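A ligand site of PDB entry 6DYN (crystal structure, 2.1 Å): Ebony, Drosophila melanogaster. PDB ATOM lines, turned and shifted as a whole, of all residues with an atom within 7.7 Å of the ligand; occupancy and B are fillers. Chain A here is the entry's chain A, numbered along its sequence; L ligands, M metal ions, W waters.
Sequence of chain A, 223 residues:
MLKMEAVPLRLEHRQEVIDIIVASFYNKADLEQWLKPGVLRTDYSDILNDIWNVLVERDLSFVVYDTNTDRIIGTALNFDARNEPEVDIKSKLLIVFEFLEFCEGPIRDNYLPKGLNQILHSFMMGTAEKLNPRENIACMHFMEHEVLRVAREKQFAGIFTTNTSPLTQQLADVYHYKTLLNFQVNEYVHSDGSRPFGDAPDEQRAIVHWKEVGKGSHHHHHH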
ATOM      1  N   PHE A  25       9.641  -7.819  10.730  1.00  0.00           N
ATOM      2  CA  PHE A  25       8.516  -8.500  10.102  1.00  0.00           C
ATOM      3  C   PHE A  25       8.325  -8.144   8.641  1.00  0.00           C
ATOM      4  O   PHE A  25       8.064  -9.045   7.841  1.00  0.00           O
ATOM      5  CB  PHE A  25       7.234  -8.221  10.873  1.00  0.00           C
ATOM      6  CG  PHE A  25       7.073  -9.056  12.113  1.00  0.00           C
ATOM      7  CD1 PHE A  25       7.827  -8.805  13.246  1.00  0.00           C
ATOM      8  CD2 PHE A  25       6.155 -10.106  12.146  1.00  0.00           C
ATOM      9  CE1 PHE A  25       7.694  -9.581  14.398  1.00  0.00           C
ATOM     10  CE2 PHE A  25       6.003 -10.880  13.287  1.00  0.00           C
ATOM     11  CZ  PHE A  25       6.776 -10.619  14.423  1.00  0.00           C
ATOM     12  N   ALA A  29       8.339 -11.808   7.367  1.00  0.00           N
ATOM     13  CA  ALA A  29       7.379 -12.678   8.026  1.00  0.00           C
ATOM     14  C   ALA A  29       6.882 -13.778   7.103  1.00  0.00           C
ATOM     15  O   ALA A  29       6.555 -13.546   5.933  1.00  0.00           O
ATOM     16  CB  ALA A  29       6.219 -11.839   8.564  1.00  0.00           C
ATOM     17  N   ASP A  30       6.804 -15.001   7.647  1.00  0.00           N
ATOM     18  CA  ASP A  30       6.571 -16.171   6.816  1.00  0.00           C
ATOM     19  C   ASP A  30       5.133 -16.255   6.312  1.00  0.00           C
ATOM     20  O   ASP A  30       4.889 -16.895   5.279  1.00  0.00           O
ATOM     21  CB  ASP A  30       6.962 -17.425   7.600  1.00  0.00           C
ATOM     22  CG  ASP A  30       8.413 -17.387   8.086  1.00  0.00           C
ATOM     23  OD1 ASP A  30       8.717 -16.564   8.977  1.00  0.00           O
ATOM     24  OD2 ASP A  30       9.238 -18.196   7.586  1.00  0.00           O
ATOM     25  N   LEU A  31       4.174 -15.663   7.001  1.00  0.00           N
ATOM     26  CA  LEU A  31       2.781 -15.713   6.539  1.00  0.00           C
ATOM     27  C   LEU A  31       2.487 -14.565   5.588  1.00  0.00           C
ATOM     28  O   LEU A  31       1.919 -14.779   4.510  1.00  0.00           O
ATOM     29  CB  LEU A  31       1.817 -15.678   7.719  1.00  0.00           C
ATOM     30  CG  LEU A  31       1.848 -16.861   8.691  1.00  0.00           C
ATOM     31  CD1 LEU A  31       0.959 -16.569   9.879  1.00  0.00           C
ATOM     32  CD2 LEU A  31       1.393 -18.126   7.994  1.00  0.00           C
ATOM     33  N   GLU A  32       2.894 -13.358   5.951  1.00  0.00           N
ATOM     34  CA  GLU A  32       2.582 -12.165   5.182  1.00  0.00           C
ATOM     35  C   GLU A  32       3.176 -12.189   3.775  1.00  0.00           C
ATOM     36  O   GLU A  32       2.663 -11.490   2.888  1.00  0.00           O
ATOM     37  CB  GLU A  32       3.064 -10.916   5.918  1.00  0.00           C
ATOM     38  CG  GLU A  32       2.288 -10.646   7.184  1.00  0.00           C
ATOM     39  CD  GLU A  32       2.858 -11.342   8.425  1.00  0.00           C
ATOM     40  OE1 GLU A  32       3.228 -12.538   8.349  1.00  0.00           O
ATOM     41  OE2 GLU A  32       2.937 -10.674   9.490  1.00  0.00           O
ATOM     42  N   TYR A  44       1.990  -2.704  10.027  1.00  0.00           N
ATOM     43  CA  TYR A  44       2.490  -3.149  11.323  1.00  0.00           C
ATOM     44  C   TYR A  44       2.537  -1.998  12.319  1.00  0.00           C
ATOM     45  O   TYR A  44       2.101  -2.152  13.468  1.00  0.00           O
ATOM     46  CB  TYR A  44       3.873  -3.779  11.156  1.00  0.00           C
ATOM     47  CG  TYR A  44       3.945  -5.023  10.295  1.00  0.00           C
ATOM     48  CD1 TYR A  44       3.521  -6.256  10.775  1.00  0.00           C
ATOM     49  CD2 TYR A  44       4.465  -4.952   9.014  1.00  0.00           C
ATOM     50  CE1 TYR A  44       3.615  -7.392   9.990  1.00  0.00           C
ATOM     51  CE2 TYR A  44       4.570  -6.086   8.220  1.00  0.00           C
ATOM     52  CZ  TYR A  44       4.135  -7.300   8.703  1.00  0.00           C
ATOM     53  OH  TYR A  44       4.260  -8.410   7.896  1.00  0.00           O
ATOM     54  N   LEU A  93      -3.256  -7.581   7.115  1.00  0.00           N
ATOM     55  CA  LEU A  93      -2.841  -8.313   8.304  1.00  0.00           C
ATOM     56  C   LEU A  93      -4.013  -8.931   9.037  1.00  0.00           C
ATOM     57  O   LEU A  93      -3.810  -9.849   9.842  1.00  0.00           O
ATOM     58  CB  LEU A  93      -2.062  -7.381   9.249  1.00  0.00           C
ATOM     59  CG  LEU A  93      -0.697  -6.903   8.741  1.00  0.00           C
ATOM     60  CD1 LEU A  93       0.082  -6.205   9.833  1.00  0.00           C
ATOM     61  CD2 LEU A  93       0.079  -8.058   8.177  1.00  0.00           C
ATOM     62  N   VAL A  96      -4.038 -12.572   8.716  1.00  0.00           N
ATOM     63  CA  VAL A  96      -3.028 -13.240   9.542  1.00  0.00           C
ATOM     64  C   VAL A  96      -3.558 -13.450  10.958  1.00  0.00           C
ATOM     65  O   VAL A  96      -3.450 -14.539  11.525  1.00  0.00           O
ATOM     66  CB  VAL A  96      -1.706 -12.457   9.542  1.00  0.00           C
ATOM     67  CG1 VAL A  96      -0.795 -12.958  10.639  1.00  0.00           C
ATOM     68  CG2 VAL A  96      -1.016 -12.603   8.202  1.00  0.00           C
ATOM     69  N   PHE A  97      -4.163 -12.404  11.535  1.00  0.00           N
ATOM     70  CA  PHE A  97      -4.680 -12.521  12.899  1.00  0.00           C
ATOM     71  C   PHE A  97      -5.864 -13.476  12.968  1.00  0.00           C
ATOM     72  O   PHE A  97      -6.002 -14.217  13.943  1.00  0.00           O
ATOM     73  CB  PHE A  97      -5.047 -11.155  13.451  1.00  0.00           C
ATOM     74  CG  PHE A  97      -3.859 -10.314  13.799  1.00  0.00           C
ATOM     75  CD1 PHE A  97      -3.292 -10.380  15.055  1.00  0.00           C
ATOM     76  CD2 PHE A  97      -3.262  -9.498  12.840  1.00  0.00           C
ATOM     77  CE1 PHE A  97      -2.170  -9.616  15.372  1.00  0.00           C
ATOM     78  CE2 PHE A  97      -2.140  -8.735  13.157  1.00  0.00           C
ATOM     79  CZ  PHE A  97      -1.595  -8.784  14.425  1.00  0.00           C
ATOM     80  N   LEU A 100      -4.364 -16.823  12.936  1.00  0.00           N
ATOM     81  CA  LEU A 100      -3.764 -17.169  14.221  1.00  0.00           C
ATOM     82  C   LEU A 100      -4.828 -17.526  15.251  1.00  0.00           C
ATOM     83  O   LEU A 100      -4.662 -18.471  16.027  1.00  0.00           O
ATOM     84  CB  LEU A 100      -2.878 -16.014  14.729  1.00  0.00           C
ATOM     85  CG  LEU A 100      -1.601 -15.741  13.905  1.00  0.00           C
ATOM     86  CD1 LEU A 100      -0.828 -14.533  14.434  1.00  0.00           C
ATOM     87  CD2 LEU A 100      -0.703 -16.959  13.882  1.00  0.00           C
ATOM     88  N   GLU A 104      -5.218 -20.696  17.462  1.00  0.00           N
ATOM     89  CA  GLU A 104      -5.215 -20.557  18.915  1.00  0.00           C
ATOM     90  C   GLU A 104      -6.519 -20.674  19.675  1.00  0.00           C
ATOM     91  O   GLU A 104      -6.583 -21.331  20.704  1.00  0.00           O
ATOM     92  CB  GLU A 104      -4.541 -19.230  19.295  1.00  0.00           C
ATOM     93  CG  GLU A 104      -3.113 -19.071  18.810  1.00  0.00           C
ATOM     94  CD  GLU A 104      -2.555 -17.674  19.020  1.00  0.00           C
ATOM     95  OE1 GLU A 104      -3.329 -16.743  19.273  1.00  0.00           O
ATOM     96  OE2 GLU A 104      -1.326 -17.503  18.950  1.00  0.00           O
ATOM     97  N   HIS A 121       0.458 -14.665  26.742  1.00  0.00           N
ATOM     98  CA  HIS A 121       0.495 -14.750  25.284  1.00  0.00           C
ATOM     99  C   HIS A 121       1.724 -13.992  24.779  1.00  0.00           C
ATOM    100  O   HIS A 121       1.783 -12.765  24.879  1.00  0.00           O
ATOM    101  CB  HIS A 121      -0.774 -14.163  24.664  1.00  0.00           C
ATOM    102  CG  HIS A 121      -0.922 -14.446  23.190  1.00  0.00           C
ATOM    103  ND1 HIS A 121      -1.622 -13.619  22.343  1.00  0.00           N
ATOM    104  CD2 HIS A 121      -0.461 -15.471  22.430  1.00  0.00           C
ATOM    105  CE1 HIS A 121      -1.589 -14.109  21.120  1.00  0.00           C
ATOM    106  NE2 HIS A 121      -0.898 -15.242  21.147  1.00  0.00           N
ATOM    107  N   SER A 122       2.682 -14.736  24.233  1.00  0.00           N
ATOM    108  CA  SER A 122       3.830 -14.129  23.547  1.00  0.00           C
ATOM    109  C   SER A 122       3.350 -13.725  22.152  1.00  0.00           C
ATOM    110  O   SER A 122       3.207 -14.563  21.262  1.00  0.00           O
ATOM    111  CB  SER A 122       5.008 -15.084  23.489  1.00  0.00           C
ATOM    112  OG  SER A 122       6.129 -14.462  22.876  1.00  0.00           O
ATOM    113  N   PHE A 123       3.091 -12.437  21.990  1.00  0.00           N
ATOM    114  CA  PHE A 123       2.386 -11.777  20.904  1.00  0.00           C
ATOM    115  C   PHE A 123       3.332 -11.440  19.745  1.00  0.00           C
ATOM    116  O   PHE A 123       3.085 -11.789  18.587  1.00  0.00           O
ATOM    117  CB  PHE A 123       1.685 -10.546  21.510  1.00  0.00           C
ATOM    118  CG  PHE A 123       1.015  -9.623  20.542  1.00  0.00           C
ATOM    119  CD1 PHE A 123      -0.299  -9.866  20.139  1.00  0.00           C
ATOM    120  CD2 PHE A 123       1.634  -8.458  20.137  1.00  0.00           C
ATOM    121  CE1 PHE A 123      -0.957  -8.991  19.264  1.00  0.00           C
ATOM    122  CE2 PHE A 123       0.996  -7.573  19.265  1.00  0.00           C
ATOM    123  CZ  PHE A 123      -0.304  -7.840  18.829  1.00  0.00           C
ATOM    124  N   MET A 124       4.448 -10.794  20.038  1.00  0.00           N
ATOM    125  CA  MET A 124       5.460 -10.517  19.037  1.00  0.00           C
ATOM    126  C   MET A 124       6.814 -10.498  19.705  1.00  0.00           C
ATOM    127  O   MET A 124       6.929 -10.169  20.888  1.00  0.00           O
ATOM    128  CB  MET A 124       5.204  -9.185  18.301  1.00  0.00           C
ATOM    129  CG  MET A 124       4.500  -9.359  16.943  1.00  0.00           C
ATOM    130  SD  MET A 124       4.318  -7.885  15.914  1.00  0.00           S
ATOM    131  CE  MET A 124       3.121  -6.926  16.821  1.00  0.00           C
ATOM    132  N   MET A 125       7.826 -10.913  18.954  1.00  0.00           N
ATOM    133  CA  MET A 125       9.227 -10.780  19.311  1.00  0.00           C
ATOM    134  C   MET A 125       9.983 -10.256  18.102  1.00  0.00           C
ATOM    135  O   MET A 125       9.560 -10.442  16.961  1.00  0.00           O
ATOM    136  CB  MET A 125       9.843 -12.077  19.738  1.00  0.00           C
ATOM    137  CG  MET A 125      10.071 -12.218  21.205  1.00  0.00           C
ATOM    138  SD  MET A 125      10.928 -13.760  21.573  1.00  0.00           S
ATOM    139  CE  MET A 125      10.196 -14.153  23.149  1.00  0.00           C
ATOM    140  N   PHE A 160       2.140 -19.065  25.939  1.00  0.00           N
ATOM    141  CA  PHE A 160       1.328 -19.525  24.820  1.00  0.00           C
ATOM    142  C   PHE A 160       1.746 -18.699  23.622  1.00  0.00           C
ATOM    143  O   PHE A 160       1.708 -17.468  23.684  1.00  0.00           O
ATOM    144  CB  PHE A 160      -0.154 -19.311  25.161  1.00  0.00           C
ATOM    145  CG  PHE A 160      -1.135 -19.829  24.149  1.00  0.00           C
ATOM    146  CD1 PHE A 160      -1.137 -21.162  23.776  1.00  0.00           C
ATOM    147  CD2 PHE A 160      -2.138 -18.999  23.644  1.00  0.00           C
ATOM    148  CE1 PHE A 160      -2.089 -21.650  22.875  1.00  0.00           C
ATOM    149  CE2 PHE A 160      -3.081 -19.479  22.755  1.00  0.00           C
ATOM    150  CZ  PHE A 160      -3.040 -20.828  22.363  1.00  0.00           C
ATOM    151  N   THR A 161       2.151 -19.355  22.532  1.00  0.00           N
ATOM    152  CA  THR A 161       2.560 -18.623  21.344  1.00  0.00           C
ATOM    153  C   THR A 161       2.348 -19.500  20.123  1.00  0.00           C
ATOM    154  O   THR A 161       2.391 -20.731  20.216  1.00  0.00           O
ATOM    155  CB  THR A 161       4.039 -18.159  21.437  1.00  0.00           C
ATOM    156  OG1 THR A 161       4.348 -17.304  20.327  1.00  0.00           O
ATOM    157  CG2 THR A 161       4.988 -19.342  21.405  1.00  0.00           C
ATOM    158  N   THR A 162       2.101 -18.853  18.983  1.00  0.00           N
ATOM    159  CA  THR A 162       2.092 -19.535  17.696  1.00  0.00           C
ATOM    160  C   THR A 162       3.379 -19.169  16.964  1.00  0.00           C
ATOM    161  O   THR A 162       3.598 -17.996  16.648  1.00  0.00           O
ATOM    162  CB  THR A 162       0.858 -19.179  16.859  1.00  0.00           C
ATOM    163  OG1 THR A 162      -0.302 -19.496  17.623  1.00  0.00           O
ATOM    164  CG2 THR A 162       0.789 -20.023  15.606  1.00  0.00           C
ATOM    165  N   ASN A 163       4.215 -20.158  16.705  1.00  0.00           N
ATOM    166  CA  ASN A 163       5.506 -19.932  16.067  1.00  0.00           C
ATOM    167  C   ASN A 163       5.398 -20.244  14.591  1.00  0.00           C
ATOM    168  O   ASN A 163       4.981 -21.358  14.216  1.00  0.00           O
ATOM    169  CB  ASN A 163       6.591 -20.754  16.756  1.00  0.00           C
ATOM    170  CG  ASN A 163       7.010 -20.113  18.070  1.00  0.00           C
ATOM    171  OD1 ASN A 163       7.306 -18.937  18.110  1.00  0.00           O
ATOM    172  ND2 ASN A 163       6.973 -20.871  19.153  1.00  0.00           N
ATOM    173  N   THR A 164       5.740 -19.267  13.745  1.00  0.00           N
ATOM    174  CA  THR A 164       5.483 -19.347  12.312  1.00  0.00           C
ATOM    175  C   THR A 164       6.758 -19.387  11.466  1.00  0.00           C
ATOM    176  O   THR A 164       6.663 -19.451  10.236  1.00  0.00           O
ATOM    177  CB  THR A 164       4.610 -18.167  11.859  1.00  0.00           C
ATOM    178  OG1 THR A 164       5.199 -16.960  12.310  1.00  0.00           O
ATOM    179  CG2 THR A 164       3.192 -18.285  12.446  1.00  0.00           C
ATOM    180  N   SER A 165       7.926 -19.344  12.081  1.00  0.00           N
ATOM    181  CA  SER A 165       9.136 -19.513  11.305  1.00  0.00           C
ATOM    182  C   SER A 165       9.913 -20.711  11.828  1.00  0.00           C
ATOM    183  O   SER A 165       9.760 -21.092  12.997  1.00  0.00           O
ATOM    184  CB  SER A 165      10.031 -18.268  11.371  1.00  0.00           C
ATOM    185  OG  SER A 165      10.686 -18.178  12.626  1.00  0.00           O
ATOM    186  N   THR A 168      11.998 -19.879  15.154  1.00  0.00           N
ATOM    187  CA  THR A 168      11.247 -19.748  16.403  1.00  0.00           C
ATOM    188  C   THR A 168      10.601 -21.064  16.796  1.00  0.00           C
ATOM    189  O   THR A 168      10.456 -21.357  17.983  1.00  0.00           O
ATOM    190  CB  THR A 168      10.190 -18.659  16.325  1.00  0.00           C
ATOM    191  OG1 THR A 168       9.315 -18.884  15.197  1.00  0.00           O
ATOM    192  CG2 THR A 168      10.843 -17.245  16.260  1.00  0.00           C
ATOM    193  N   ALA A 206       2.370 -23.572  10.972  1.00  0.00           N
ATOM    194  CA  ALA A 206       2.146 -22.719  12.129  1.00  0.00           C
ATOM    195  C   ALA A 206       1.994 -23.671  13.295  1.00  0.00           C
ATOM    196  O   ALA A 206       1.138 -24.556  13.275  1.00  0.00           O
ATOM    197  CB  ALA A 206       0.899 -21.835  11.971  1.00  0.00           C
ATOM    198  N   ILE A 207       2.853 -23.522  14.293  1.00  0.00           N
ATOM    199  CA  ILE A 207       2.875 -24.440  15.420  1.00  0.00           C
ATOM    200  C   ILE A 207       2.474 -23.663  16.668  1.00  0.00           C
ATOM    201  O   ILE A 207       3.088 -22.634  16.993  1.00  0.00           O
ATOM    202  CB  ILE A 207       4.247 -25.108  15.592  1.00  0.00           C
ATOM    203  CG1 ILE A 207       4.594 -25.854  14.283  1.00  0.00           C
ATOM    204  CG2 ILE A 207       4.214 -26.038  16.773  1.00  0.00           C
ATOM    205  CD1 ILE A 207       6.005 -26.372  14.223  1.00  0.00           C
HETATM  206  N1  LIG L   1       3.382 -14.914  16.864  1.00  0.00           N
HETATM  207  C1  LIG L   1       2.615 -15.149  15.652  1.00  0.00           C
HETATM  208  C2  LIG L   1       3.551 -15.066  14.431  1.00  0.00           C
HETATM  209  C3  LIG L   1       3.169 -13.864  13.555  1.00  0.00           C
HETATM  210  N2  LIG L   1       2.705 -12.703  13.994  1.00  0.00           N
HETATM  211  C4  LIG L   1       3.275 -13.781  12.188  1.00  0.00           C
HETATM  212  C5  LIG L   1       2.500 -11.915  12.917  1.00  0.00           C
HETATM  213  N3  LIG L   1       2.856 -12.590  11.818  1.00  0.00           N
HETATM  214 CA    CA M   1       7.460 -17.077  19.658  1.00  0.00          CA
HETATM  215  O   HOH W   1       2.018 -15.949  19.195  1.00  0.00           O
HETATM  216  O   HOH W   2      -0.177 -15.361  17.735  1.00  0.00           O
HETATM  217  O   HOH W   3       6.078 -16.048  17.469  1.00  0.00           O
HETATM  218  O   HOH W   4       4.281 -14.528   9.617  1.00  0.00           O
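O of Thr 162 lies within hydrogen-bond range of N1 of the ligand, at 3.1 Å.
A nitrogen (N3) of the ligand sits at hydrogen-bond distance from the side-chain carboxylate of Glu 32, at 3.0 Å.
The side-chain carboxylate (OE2) of Glu 32 lies close to the side-chain hydroxyl (OH) of Tyr 44 (3.1 Å).
OG1 of Thr 162 is in hydrogen-bond range of OE2 of Glu 104 (2.6 Å).
Phe 25 touches the ligand (CE2 to C5, 3.7 Å).
Val 96 touches the ligand (CG1 to N3, 3.9 Å).
Leu 100 touches the ligand.
Phe 123 touches the ligand.
Thr 164 touches the ligand (OG1 to C2, 3.3 Å).
Hydrophobic or aromatic side chains that line the ligand: Phe 25, Val 96 and Leu 100.
Water W4 lies within hydrogen-bond range of the side-chain carboxylate (OE1) of Glu 32, the backbone NH (N) of Leu 31, the backbone NH (N) of Asp 30 and a nitrogen (N3) of the ligand.
Water W1 lies within hydrogen-bond range of O of Ser 122 (2.8 Å), N1 of the ligand (2.9 Å), N of Thr 162 (2.9 Å) and OG1 of Thr 161 (2.9 Å).
Water W3 bridges N1 of the ligand and O of Thr 162.
Water W2 lies within hydrogen-bond range of OE2 of Glu 104 (2.7 Å) and NE2 of His 121 (3.5 Å).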
